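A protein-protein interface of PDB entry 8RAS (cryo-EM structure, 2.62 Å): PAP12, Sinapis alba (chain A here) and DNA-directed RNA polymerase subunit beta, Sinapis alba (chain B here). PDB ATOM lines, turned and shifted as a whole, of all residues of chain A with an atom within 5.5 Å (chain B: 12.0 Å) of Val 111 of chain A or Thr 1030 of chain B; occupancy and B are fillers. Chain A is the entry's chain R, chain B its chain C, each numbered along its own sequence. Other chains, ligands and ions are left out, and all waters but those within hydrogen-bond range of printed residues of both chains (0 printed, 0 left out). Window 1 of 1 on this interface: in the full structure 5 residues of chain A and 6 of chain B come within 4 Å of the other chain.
O of Thr 1024 of chain B lies within hydrogen-bond range of N of Gly 1029 of chain B (3.1 Å).
Among the printed residues, merely in contact across the chains: Thr 108 of chain A with Thr 1030 of chain B, Val 111 of chain A with Gly 1028 of chain B, Val 111 of chain A with Thr 1030 of chain B, Arg 115 of chain A with Ile 1027 of chain B, Arg 115 of chain A with Gly 1028 of chain B and Arg 115 of chain A with Gly 1029 of chain B.
No residue of chain B comes within 4 Å of Ala 107 of chain A. Printed residues of chain B within 4 Å of Thr 108 of chain A: Thr 1030 (3.99 Å). Of chain B, only Gly 1028 (3.8 Å) and Thr 1030 (3.4 Å) come within 4 Å of Val 111 of chain A. Lys 113 of chain A touches none of the printed residues of chain B. Asn 114 of chain A touches none of the printed residues of chain B. No residue of chain B comes within 4 Å of Tyr 118 of chain A. No residue of chain B comes within 4 Å of Ala 124 of chain A. Printed residues of chain A within 4 Å of Ile 1027 of chain B: Arg 115 (3.3 Å). Of the printed residues of chain A, Gly 1028 of chain B touches Val 111 and Arg 115. Of the printed residues of chain A, Gly 1029 of chain B touches Arg 115 (3.5 Å). Printed residues of chain A within 4 Å of Thr 1030 of chain B: Thr 108 and Val 111.
Printed residues of chain A that touch a printed residue of chain B: Thr 108, Val 111 and Arg 115. Hydrophobic or aromatic side chains of chain A that line the printed part of chain B: Val 111. Among the printed residues, no Asp or Glu carboxylate lies within 4 Å of a Lys or Arg side-chain nitrogen of the other chain.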
ATOM      1  N   GLU A 106     -10.213  -0.868 -17.290  1.00  0.00           N
ATOM      2  CA  GLU A 106      -9.183  -1.882 -17.087  1.00  0.00           C
ATOM      3  C   GLU A 106      -7.900  -1.265 -16.544  1.00  0.00           C
ATOM      4  O   GLU A 106      -7.253  -1.838 -15.657  1.00  0.00           O
ATOM      5  CB  GLU A 106      -8.917  -2.625 -18.394  1.00  0.00           C
ATOM      6  CG  GLU A 106      -8.232  -3.965 -18.212  1.00  0.00           C
ATOM      7  CD  GLU A 106      -8.045  -4.701 -19.520  1.00  0.00           C
ATOM      8  OE1 GLU A 106      -8.791  -4.411 -20.477  1.00  0.00           O
ATOM      9  OE2 GLU A 106      -7.151  -5.569 -19.594  1.00  0.00           O
ATOM     10  N   ALA A 107      -7.514  -0.096 -17.060  1.00  0.00           N
ATOM     11  CA  ALA A 107      -6.334   0.588 -16.542  1.00  0.00           C
ATOM     12  C   ALA A 107      -6.528   0.996 -15.087  1.00  0.00           C
ATOM     13  O   ALA A 107      -5.593   0.913 -14.280  1.00  0.00           O
ATOM     14  CB  ALA A 107      -6.011   1.807 -17.404  1.00  0.00           C
ATOM     15  N   THR A 108      -7.733   1.451 -14.736  1.00  0.00           N
ATOM     16  CA  THR A 108      -8.018   1.796 -13.349  1.00  0.00           C
ATOM     17  C   THR A 108      -7.884   0.579 -12.444  1.00  0.00           C
ATOM     18  O   THR A 108      -7.307   0.668 -11.355  1.00  0.00           O
ATOM     19  CB  THR A 108      -9.418   2.399 -13.238  1.00  0.00           C
ATOM     20  OG1 THR A 108      -9.455   3.652 -13.931  1.00  0.00           O
ATOM     21  CG2 THR A 108      -9.791   2.624 -11.784  1.00  0.00           C
ATOM     22  N   GLU A 109      -8.406  -0.568 -12.883  1.00  0.00           N
ATOM     23  CA  GLU A 109      -8.249  -1.792 -12.100  1.00  0.00           C
ATOM     24  C   GLU A 109      -6.778  -2.160 -11.945  1.00  0.00           C
ATOM     25  O   GLU A 109      -6.341  -2.560 -10.858  1.00  0.00           O
ATOM     26  CB  GLU A 109      -9.019  -2.940 -12.750  1.00  0.00           C
ATOM     27  CG  GLU A 109     -10.523  -2.756 -12.758  1.00  0.00           C
ATOM     28  CD  GLU A 109     -11.218  -3.745 -13.670  1.00  0.00           C
ATOM     29  OE1 GLU A 109     -10.524  -4.594 -14.267  1.00  0.00           O
ATOM     30  OE2 GLU A 109     -12.460  -3.674 -13.791  1.00  0.00           O
ATOM     31  N   TYR A 110      -6.000  -2.033 -13.025  1.00  0.00           N
ATOM     32  CA  TYR A 110      -4.568  -2.304 -12.948  1.00  0.00           C
ATOM     33  C   TYR A 110      -3.895  -1.418 -11.910  1.00  0.00           C
ATOM     34  O   TYR A 110      -3.072  -1.890 -11.118  1.00  0.00           O
ATOM     35  CB  TYR A 110      -3.909  -2.091 -14.311  1.00  0.00           C
ATOM     36  CG  TYR A 110      -4.124  -3.195 -15.319  1.00  0.00           C
ATOM     37  CD1 TYR A 110      -5.038  -4.212 -15.090  1.00  0.00           C
ATOM     38  CD2 TYR A 110      -3.402  -3.219 -16.504  1.00  0.00           C
ATOM     39  CE1 TYR A 110      -5.231  -5.218 -16.015  1.00  0.00           C
ATOM     40  CE2 TYR A 110      -3.586  -4.219 -17.431  1.00  0.00           C
ATOM     41  CZ  TYR A 110      -4.501  -5.215 -17.184  1.00  0.00           C
ATOM     42  OH  TYR A 110      -4.685  -6.215 -18.111  1.00  0.00           O
ATOM     43  N   VAL A 111      -4.228  -0.127 -11.907  1.00  0.00           N
ATOM     44  CA  VAL A 111      -3.587   0.800 -10.977  1.00  0.00           C
ATOM     45  C   VAL A 111      -3.993   0.492  -9.542  1.00  0.00           C
ATOM     46  O   VAL A 111      -3.158   0.517  -8.631  1.00  0.00           O
ATOM     47  CB  VAL A 111      -3.910   2.254 -11.362  1.00  0.00           C
ATOM     48  CG1 VAL A 111      -3.464   3.204 -10.266  1.00  0.00           C
ATOM     49  CG2 VAL A 111      -3.230   2.608 -12.663  1.00  0.00           C
ATOM     50  N   GLU A 112      -5.275   0.200  -9.310  1.00  0.00           N
ATOM     51  CA  GLU A 112      -5.711  -0.104  -7.950  1.00  0.00           C
ATOM     52  C   GLU A 112      -5.069  -1.385  -7.428  1.00  0.00           C
ATOM     53  O   GLU A 112      -4.692  -1.461  -6.254  1.00  0.00           O
ATOM     54  CB  GLU A 112      -7.236  -0.201  -7.880  1.00  0.00           C
ATOM     55  CG  GLU A 112      -7.964   1.005  -8.440  1.00  0.00           C
ATOM     56  CD  GLU A 112      -9.036   1.526  -7.508  1.00  0.00           C
ATOM     57  OE1 GLU A 112      -8.702   1.896  -6.364  1.00  0.00           O
ATOM     58  OE2 GLU A 112     -10.215   1.566  -7.921  1.00  0.00           O
ATOM     59  N   LYS A 113      -4.936  -2.404  -8.282  1.00  0.00           N
ATOM     60  CA  LYS A 113      -4.373  -3.670  -7.819  1.00  0.00           C
ATOM     61  C   LYS A 113      -2.892  -3.536  -7.484  1.00  0.00           C
ATOM     62  O   LYS A 113      -2.450  -3.960  -6.410  1.00  0.00           O
ATOM     63  CB  LYS A 113      -4.594  -4.758  -8.868  1.00  0.00           C
ATOM     64  CG  LYS A 113      -5.754  -5.687  -8.549  1.00  0.00           C
ATOM     65  CD  LYS A 113      -6.368  -6.262  -9.811  1.00  0.00           C
ATOM     66  CE  LYS A 113      -7.848  -6.546  -9.616  1.00  0.00           C
ATOM     67  NZ  LYS A 113      -8.604  -5.306  -9.287  1.00  0.00           N
ATOM     68  N   ASN A 114      -2.106  -2.948  -8.386  1.00  0.00           N
ATOM     69  CA  ASN A 114      -0.658  -2.792  -8.201  1.00  0.00           C
ATOM     70  C   ASN A 114      -0.301  -1.337  -8.485  1.00  0.00           C
ATOM     71  O   ASN A 114       0.041  -0.982  -9.615  1.00  0.00           O
ATOM     72  CB  ASN A 114       0.115  -3.748  -9.101  1.00  0.00           C
ATOM     73  CG  ASN A 114      -0.660  -5.009  -9.416  1.00  0.00           C
ATOM     74  OD1 ASN A 114      -1.271  -5.127 -10.477  1.00  0.00           O
ATOM     75  ND2 ASN A 114      -0.641  -5.962  -8.491  1.00  0.00           N
ATOM     76  N   ARG A 115      -0.371  -0.500  -7.449  1.00  0.00           N
ATOM     77  CA  ARG A 115      -0.189   0.936  -7.635  1.00  0.00           C
ATOM     78  C   ARG A 115       1.245   1.285  -8.016  1.00  0.00           C
ATOM     79  O   ARG A 115       1.470   2.117  -8.902  1.00  0.00           O
ATOM     80  CB  ARG A 115      -0.600   1.676  -6.364  1.00  0.00           C
ATOM     81  CG  ARG A 115      -0.387   3.173  -6.420  1.00  0.00           C
ATOM     82  CD  ARG A 115      -0.441   3.783  -5.033  1.00  0.00           C
ATOM     83  NE  ARG A 115      -1.788   4.219  -4.685  1.00  0.00           N
ATOM     84  CZ  ARG A 115      -2.149   4.647  -3.483  1.00  0.00           C
ATOM     85  NH1 ARG A 115      -1.283   4.708  -2.483  1.00  0.00           N
ATOM     86  NH2 ARG A 115      -3.408   5.023  -3.279  1.00  0.00           N
ATOM     87  N   TYR A 118       3.227   1.275 -11.820  1.00  0.00           N
ATOM     88  CA  TYR A 118       2.868   2.155 -12.918  1.00  0.00           C
ATOM     89  C   TYR A 118       3.259   3.590 -12.596  1.00  0.00           C
ATOM     90  O   TYR A 118       3.579   3.937 -11.456  1.00  0.00           O
ATOM     91  CB  TYR A 118       1.368   2.063 -13.220  1.00  0.00           C
ATOM     92  CG  TYR A 118       0.900   0.657 -13.499  1.00  0.00           C
ATOM     93  CD1 TYR A 118       1.176   0.040 -14.709  1.00  0.00           C
ATOM     94  CD2 TYR A 118       0.190  -0.057 -12.548  1.00  0.00           C
ATOM     95  CE1 TYR A 118       0.753  -1.245 -14.966  1.00  0.00           C
ATOM     96  CE2 TYR A 118      -0.237  -1.344 -12.796  1.00  0.00           C
ATOM     97  CZ  TYR A 118       0.049  -1.933 -14.006  1.00  0.00           C
ATOM     98  OH  TYR A 118      -0.375  -3.216 -14.259  1.00  0.00           O
ATOM     99  N   ALA A 124      -0.240   2.358 -17.284  1.00  0.00           N
ATOM    100  CA  ALA A 124      -1.371   1.444 -17.153  1.00  0.00           C
ATOM    101  C   ALA A 124      -2.128   1.289 -18.466  1.00  0.00           C
ATOM    102  O   ALA A 124      -2.511   0.175 -18.838  1.00  0.00           O
ATOM    103  CB  ALA A 124      -2.311   1.928 -16.053  1.00  0.00           C
ATOM    104  N   HIS B1002     -14.755  13.087 -20.579  1.00  0.00           N
ATOM    105  CA  HIS B1002     -14.009  13.077 -19.328  1.00  0.00           C
ATOM    106  C   HIS B1002     -12.863  14.077 -19.321  1.00  0.00           C
ATOM    107  O   HIS B1002     -12.479  14.557 -18.251  1.00  0.00           O
ATOM    108  CB  HIS B1002     -13.481  11.670 -19.045  1.00  0.00           C
ATOM    109  CG  HIS B1002     -14.543  10.712 -18.605  1.00  0.00           C
ATOM    110  ND1 HIS B1002     -15.093   9.773 -19.448  1.00  0.00           N
ATOM    111  CD2 HIS B1002     -15.166  10.560 -17.413  1.00  0.00           C
ATOM    112  CE1 HIS B1002     -16.005   9.077 -18.793  1.00  0.00           C
ATOM    113  NE2 HIS B1002     -16.069   9.535 -17.557  1.00  0.00           N
ATOM    114  N   GLN B1005     -14.772  17.277 -18.376  1.00  0.00           N
ATOM    115  CA  GLN B1005     -15.107  17.374 -16.960  1.00  0.00           C
ATOM    116  C   GLN B1005     -13.880  17.659 -16.107  1.00  0.00           C
ATOM    117  O   GLN B1005     -14.000  18.273 -15.041  1.00  0.00           O
ATOM    118  CB  GLN B1005     -15.792  16.094 -16.487  1.00  0.00           C
ATOM    119  CG  GLN B1005     -16.741  16.311 -15.324  1.00  0.00           C
ATOM    120  CD  GLN B1005     -16.857  15.099 -14.431  1.00  0.00           C
ATOM    121  OE1 GLN B1005     -15.988  14.229 -14.430  1.00  0.00           O
ATOM    122  NE2 GLN B1005     -17.935  15.034 -13.662  1.00  0.00           N
ATOM    123  N   GLU B1006     -12.702  17.212 -16.545  1.00  0.00           N
ATOM    124  CA  GLU B1006     -11.473  17.532 -15.827  1.00  0.00           C
ATOM    125  C   GLU B1006     -11.247  19.033 -15.778  1.00  0.00           C
ATOM    126  O   GLU B1006     -10.942  19.598 -14.721  1.00  0.00           O
ATOM    127  CB  GLU B1006     -10.281  16.852 -16.494  1.00  0.00           C
ATOM    128  CG  GLU B1006     -10.131  15.388 -16.189  1.00  0.00           C
ATOM    129  CD  GLU B1006      -8.682  14.963 -16.188  1.00  0.00           C
ATOM    130  OE1 GLU B1006      -7.930  15.411 -17.077  1.00  0.00           O
ATOM    131  OE2 GLU B1006      -8.289  14.189 -15.290  1.00  0.00           O
ATOM    132  N   TYR B1010     -12.276  20.048 -11.446  1.00  0.00           N
ATOM    133  CA  TYR B1010     -11.192  19.959 -10.473  1.00  0.00           C
ATOM    134  C   TYR B1010      -9.864  20.472 -11.004  1.00  0.00           C
ATOM    135  O   TYR B1010      -8.840  20.326 -10.330  1.00  0.00           O
ATOM    136  CB  TYR B1010     -11.051  18.532  -9.926  1.00  0.00           C
ATOM    137  CG  TYR B1010     -10.661  17.417 -10.877  1.00  0.00           C
ATOM    138  CD1 TYR B1010      -9.463  17.443 -11.580  1.00  0.00           C
ATOM    139  CD2 TYR B1010     -11.472  16.301 -11.018  1.00  0.00           C
ATOM    140  CE1 TYR B1010      -9.107  16.409 -12.421  1.00  0.00           C
ATOM    141  CE2 TYR B1010     -11.124  15.265 -11.855  1.00  0.00           C
ATOM    142  CZ  TYR B1010      -9.942  15.323 -12.552  1.00  0.00           C
ATOM    143  OH  TYR B1010      -9.597  14.286 -13.379  1.00  0.00           O
ATOM    144  N   ARG B1016     -13.035  21.243  -3.244  1.00  0.00           N
ATOM    145  CA  ARG B1016     -12.783  19.959  -2.603  1.00  0.00           C
ATOM    146  C   ARG B1016     -11.977  19.034  -3.504  1.00  0.00           C
ATOM    147  O   ARG B1016     -11.036  18.377  -3.046  1.00  0.00           O
ATOM    148  CB  ARG B1016     -14.101  19.299  -2.205  1.00  0.00           C
ATOM    149  CG  ARG B1016     -13.963  18.290  -1.078  1.00  0.00           C
ATOM    150  CD  ARG B1016     -15.150  17.344  -1.030  1.00  0.00           C
ATOM    151  NE  ARG B1016     -15.642  17.016  -2.363  1.00  0.00           N
ATOM    152  CZ  ARG B1016     -15.106  16.099  -3.155  1.00  0.00           C
ATOM    153  NH1 ARG B1016     -14.052  15.392  -2.780  1.00  0.00           N
ATOM    154  NH2 ARG B1016     -15.639  15.886  -4.355  1.00  0.00           N
ATOM    155  N   ALA B1017     -12.328  18.971  -4.789  1.00  0.00           N
ATOM    156  CA  ALA B1017     -11.681  18.034  -5.698  1.00  0.00           C
ATOM    157  C   ALA B1017     -10.336  18.530  -6.211  1.00  0.00           C
ATOM    158  O   ALA B1017      -9.548  17.724  -6.715  1.00  0.00           O
ATOM    159  CB  ALA B1017     -12.606  17.728  -6.875  1.00  0.00           C
ATOM    160  N   ARG B1018     -10.056  19.831  -6.101  1.00  0.00           N
ATOM    161  CA  ARG B1018      -8.723  20.322  -6.438  1.00  0.00           C
ATOM    162  C   ARG B1018      -7.689  19.828  -5.437  1.00  0.00           C
ATOM    163  O   ARG B1018      -6.554  19.514  -5.810  1.00  0.00           O
ATOM    164  CB  ARG B1018      -8.718  21.849  -6.491  1.00  0.00           C
ATOM    165  CG  ARG B1018      -9.234  22.435  -7.785  1.00  0.00           C
ATOM    166  CD  ARG B1018      -9.114  23.946  -7.782  1.00  0.00           C
ATOM    167  NE  ARG B1018      -9.151  24.499  -6.433  1.00  0.00           N
ATOM    168  CZ  ARG B1018      -9.737  25.644  -6.111  1.00  0.00           C
ATOM    169  NH1 ARG B1018     -10.360  26.380  -7.015  1.00  0.00           N
ATOM    170  NH2 ARG B1018      -9.690  26.064  -4.850  1.00  0.00           N
ATOM    171  N   GLN B1019      -8.062  19.762  -4.158  1.00  0.00           N
ATOM    172  CA  GLN B1019      -7.118  19.334  -3.134  1.00  0.00           C
ATOM    173  C   GLN B1019      -6.841  17.840  -3.211  1.00  0.00           C
ATOM    174  O   GLN B1019      -5.713  17.407  -2.951  1.00  0.00           O
ATOM    175  CB  GLN B1019      -7.645  19.708  -1.750  1.00  0.00           C
ATOM    176  CG  GLN B1019      -7.325  21.134  -1.338  1.00  0.00           C
ATOM    177  CD  GLN B1019      -8.533  21.872  -0.803  1.00  0.00           C
ATOM    178  OE1 GLN B1019      -9.254  21.364   0.056  1.00  0.00           O
ATOM    179  NE2 GLN B1019      -8.762  23.078  -1.307  1.00  0.00           N
ATOM    180  N   GLU B1020      -7.848  17.039  -3.561  1.00  0.00           N
ATOM    181  CA  GLU B1020      -7.644  15.597  -3.644  1.00  0.00           C
ATOM    182  C   GLU B1020      -6.836  15.212  -4.873  1.00  0.00           C
ATOM    183  O   GLU B1020      -6.064  14.248  -4.827  1.00  0.00           O
ATOM    184  CB  GLU B1020      -8.991  14.871  -3.640  1.00  0.00           C
ATOM    185  CG  GLU B1020     -10.069  15.347  -2.628  1.00  0.00           C
ATOM    186  CD  GLU B1020      -9.562  15.904  -1.286  1.00  0.00           C
ATOM    187  OE1 GLU B1020     -10.385  16.527  -0.580  1.00  0.00           O
ATOM    188  OE2 GLU B1020      -8.404  15.673  -0.881  1.00  0.00           O
ATOM    189  N   VAL B1021      -7.005  15.936  -5.981  1.00  0.00           N
ATOM    190  CA  VAL B1021      -6.193  15.676  -7.165  1.00  0.00           C
ATOM    191  C   VAL B1021      -4.726  15.959  -6.869  1.00  0.00           C
ATOM    192  O   VAL B1021      -3.832  15.241  -7.332  1.00  0.00           O
ATOM    193  CB  VAL B1021      -6.712  16.499  -8.359  1.00  0.00           C
ATOM    194  CG1 VAL B1021      -5.573  16.905  -9.277  1.00  0.00           C
ATOM    195  CG2 VAL B1021      -7.752  15.706  -9.124  1.00  0.00           C
ATOM    196  N   LEU B1022      -4.459  17.002  -6.080  1.00  0.00           N
ATOM    197  CA  LEU B1022      -3.090  17.287  -5.663  1.00  0.00           C
ATOM    198  C   LEU B1022      -2.503  16.135  -4.858  1.00  0.00           C
ATOM    199  O   LEU B1022      -1.301  15.867  -4.948  1.00  0.00           O
ATOM    200  CB  LEU B1022      -3.058  18.587  -4.852  1.00  0.00           C
ATOM    201  CG  LEU B1022      -1.744  19.358  -4.672  1.00  0.00           C
ATOM    202  CD1 LEU B1022      -0.864  18.759  -3.580  1.00  0.00           C
ATOM    203  CD2 LEU B1022      -0.988  19.436  -5.987  1.00  0.00           C
ATOM    204  N   GLY B1023      -3.327  15.439  -4.080  1.00  0.00           N
ATOM    205  CA  GLY B1023      -2.844  14.352  -3.253  1.00  0.00           C
ATOM    206  C   GLY B1023      -2.732  13.023  -3.970  1.00  0.00           C
ATOM    207  O   GLY B1023      -1.755  12.295  -3.782  1.00  0.00           O
ATOM    208  N   THR B1024      -3.733  12.688  -4.787  1.00  0.00           N
ATOM    209  CA  THR B1024      -3.719  11.406  -5.487  1.00  0.00           C
ATOM    210  C   THR B1024      -2.575  11.325  -6.488  1.00  0.00           C
ATOM    211  O   THR B1024      -1.926  10.282  -6.612  1.00  0.00           O
ATOM    212  CB  THR B1024      -5.056  11.171  -6.189  1.00  0.00           C
ATOM    213  OG1 THR B1024      -5.468  12.372  -6.851  1.00  0.00           O
ATOM    214  CG2 THR B1024      -6.119  10.760  -5.186  1.00  0.00           C
ATOM    215  N   THR B1025      -2.313  12.414  -7.217  1.00  0.00           N
ATOM    216  CA  THR B1025      -1.268  12.385  -8.235  1.00  0.00           C
ATOM    217  C   THR B1025       0.118  12.222  -7.625  1.00  0.00           C
ATOM    218  O   THR B1025       1.002  11.630  -8.253  1.00  0.00           O
ATOM    219  CB  THR B1025      -1.322  13.654  -9.085  1.00  0.00           C
ATOM    220  OG1 THR B1025      -1.678  14.768  -8.258  1.00  0.00           O
ATOM    221  CG2 THR B1025      -2.346  13.506 -10.197  1.00  0.00           C
ATOM    222  N   ILE B1026       0.329  12.740  -6.415  1.00  0.00           N
ATOM    223  CA  ILE B1026       1.613  12.567  -5.745  1.00  0.00           C
ATOM    224  C   ILE B1026       1.793  11.140  -5.242  1.00  0.00           C
ATOM    225  O   ILE B1026       2.930  10.665  -5.130  1.00  0.00           O
ATOM    226  CB  ILE B1026       1.750  13.592  -4.607  1.00  0.00           C
ATOM    227  CG1 ILE B1026       1.749  15.010  -5.179  1.00  0.00           C
ATOM    228  CG2 ILE B1026       3.026  13.373  -3.814  1.00  0.00           C
ATOM    229  CD1 ILE B1026       1.931  16.091  -4.138  1.00  0.00           C
ATOM    230  N   ILE B1027       0.702  10.429  -4.961  1.00  0.00           N
ATOM    231  CA  ILE B1027       0.771   9.023  -4.579  1.00  0.00           C
ATOM    232  C   ILE B1027       0.372   8.088  -5.707  1.00  0.00           C
ATOM    233  O   ILE B1027       0.544   6.867  -5.565  1.00  0.00           O
ATOM    234  CB  ILE B1027      -0.084   8.734  -3.327  1.00  0.00           C
ATOM    235  CG1 ILE B1027      -1.566   8.961  -3.629  1.00  0.00           C
ATOM    236  CG2 ILE B1027       0.360   9.606  -2.167  1.00  0.00           C
ATOM    237  CD1 ILE B1027      -2.480   8.596  -2.484  1.00  0.00           C
ATOM    238  N   GLY B1028      -0.144   8.609  -6.819  1.00  0.00           N
ATOM    239  CA  GLY B1028      -0.506   7.789  -7.959  1.00  0.00           C
ATOM    240  C   GLY B1028      -1.628   6.810  -7.690  1.00  0.00           C
ATOM    241  O   GLY B1028      -1.528   5.637  -8.059  1.00  0.00           O
ATOM    242  N   GLY B1029      -2.705   7.273  -7.061  1.00  0.00           N
ATOM    243  CA  GLY B1029      -3.752   6.370  -6.628  1.00  0.00           C
ATOM    244  C   GLY B1029      -5.131   6.604  -7.209  1.00  0.00           C
ATOM    245  O   GLY B1029      -6.127   6.466  -6.491  1.00  0.00           O
ATOM    246  N   THR B1030      -5.201   6.976  -8.492  1.00  0.00           N
ATOM    247  CA  THR B1030      -6.445   7.046  -9.259  1.00  0.00           C
ATOM    248  C   THR B1030      -7.344   8.195  -8.809  1.00  0.00           C
ATOM    249  O   THR B1030      -7.635   8.344  -7.618  1.00  0.00           O
ATOM    250  CB  THR B1030      -7.205   5.715  -9.188  1.00  0.00           C
ATOM    251  OG1 THR B1030      -6.493   4.716  -9.929  1.00  0.00           O
ATOM    252  CG2 THR B1030      -8.601   5.858  -9.765  1.00  0.00           C
ATOM    253  N   ILE B1031      -7.797   9.003  -9.760  1.00  0.00           N
ATOM    254  CA  ILE B1031      -8.598  10.193  -9.484  1.00  0.00           C
ATOM    255  C   ILE B1031     -10.067   9.838  -9.682  1.00  0.00           C
ATOM    256  O   ILE B1031     -10.434   9.358 -10.765  1.00  0.00           O
ATOM    257  CB  ILE B1031      -8.188  11.363 -10.390  1.00  0.00           C
ATOM    258  CG1 ILE B1031      -6.769  11.822 -10.049  1.00  0.00           C
ATOM    259  CG2 ILE B1031      -9.173  12.509 -10.258  1.00  0.00           C
ATOM    260  CD1 ILE B1031      -6.073  12.538 -11.180  1.00  0.00           C
ATOM    261  N   PRO B1032     -10.927  10.048  -8.690  1.00  0.00           N
ATOM    262  CA  PRO B1032     -12.347   9.733  -8.841  1.00  0.00           C
ATOM    263  C   PRO B1032     -13.147  10.926  -9.354  1.00  0.00           C
ATOM    264  O   PRO B1032     -12.678  12.066  -9.375  1.00  0.00           O
ATOM    265  CB  PRO B1032     -12.774   9.364  -7.412  1.00  0.00           C
ATOM    266  CG  PRO B1032     -11.730   9.988  -6.504  1.00  0.00           C
ATOM    267  CD  PRO B1032     -10.619  10.555  -7.345  1.00  0.00           C
ATOM    268  N   LYS B1033     -14.377  10.637  -9.768  1.00  0.00           N
ATOM    269  CA  LYS B1033     -15.254  11.672 -10.289  1.00  0.00           C
ATOM    270  C   LYS B1033     -15.682  12.627  -9.174  1.00  0.00           C
ATOM    271  O   LYS B1033     -15.870  12.213  -8.027  1.00  0.00           O
ATOM    272  CB  LYS B1033     -16.483  11.051 -10.943  1.00  0.00           C
ATOM    273  CG  LYS B1033     -16.401  10.971 -12.459  1.00  0.00           C
ATOM    274  CD  LYS B1033     -15.382   9.937 -12.909  1.00  0.00           C
ATOM    275  CE  LYS B1033     -15.668   8.573 -12.301  1.00  0.00           C
ATOM    276  NZ  LYS B1033     -14.450   7.718 -12.265  1.00  0.00           N
ATOM    277  N   PRO B1034     -15.845  13.917  -9.489  1.00  0.00           N
ATOM    278  CA  PRO B1034     -16.190  14.899  -8.450  1.00  0.00           C
ATOM    279  C   PRO B1034     -17.575  14.687  -7.860  1.00  0.00           C
ATOM    280  O   PRO B1034     -17.736  14.665  -6.635  1.00  0.00           O
ATOM    281  CB  PRO B1034     -16.099  16.240  -9.190  1.00  0.00           C
ATOM    282  CG  PRO B1034     -15.306  15.960 -10.425  1.00  0.00           C
ATOM    283  CD  PRO B1034     -15.628  14.554 -10.798  1.00  0.00           C
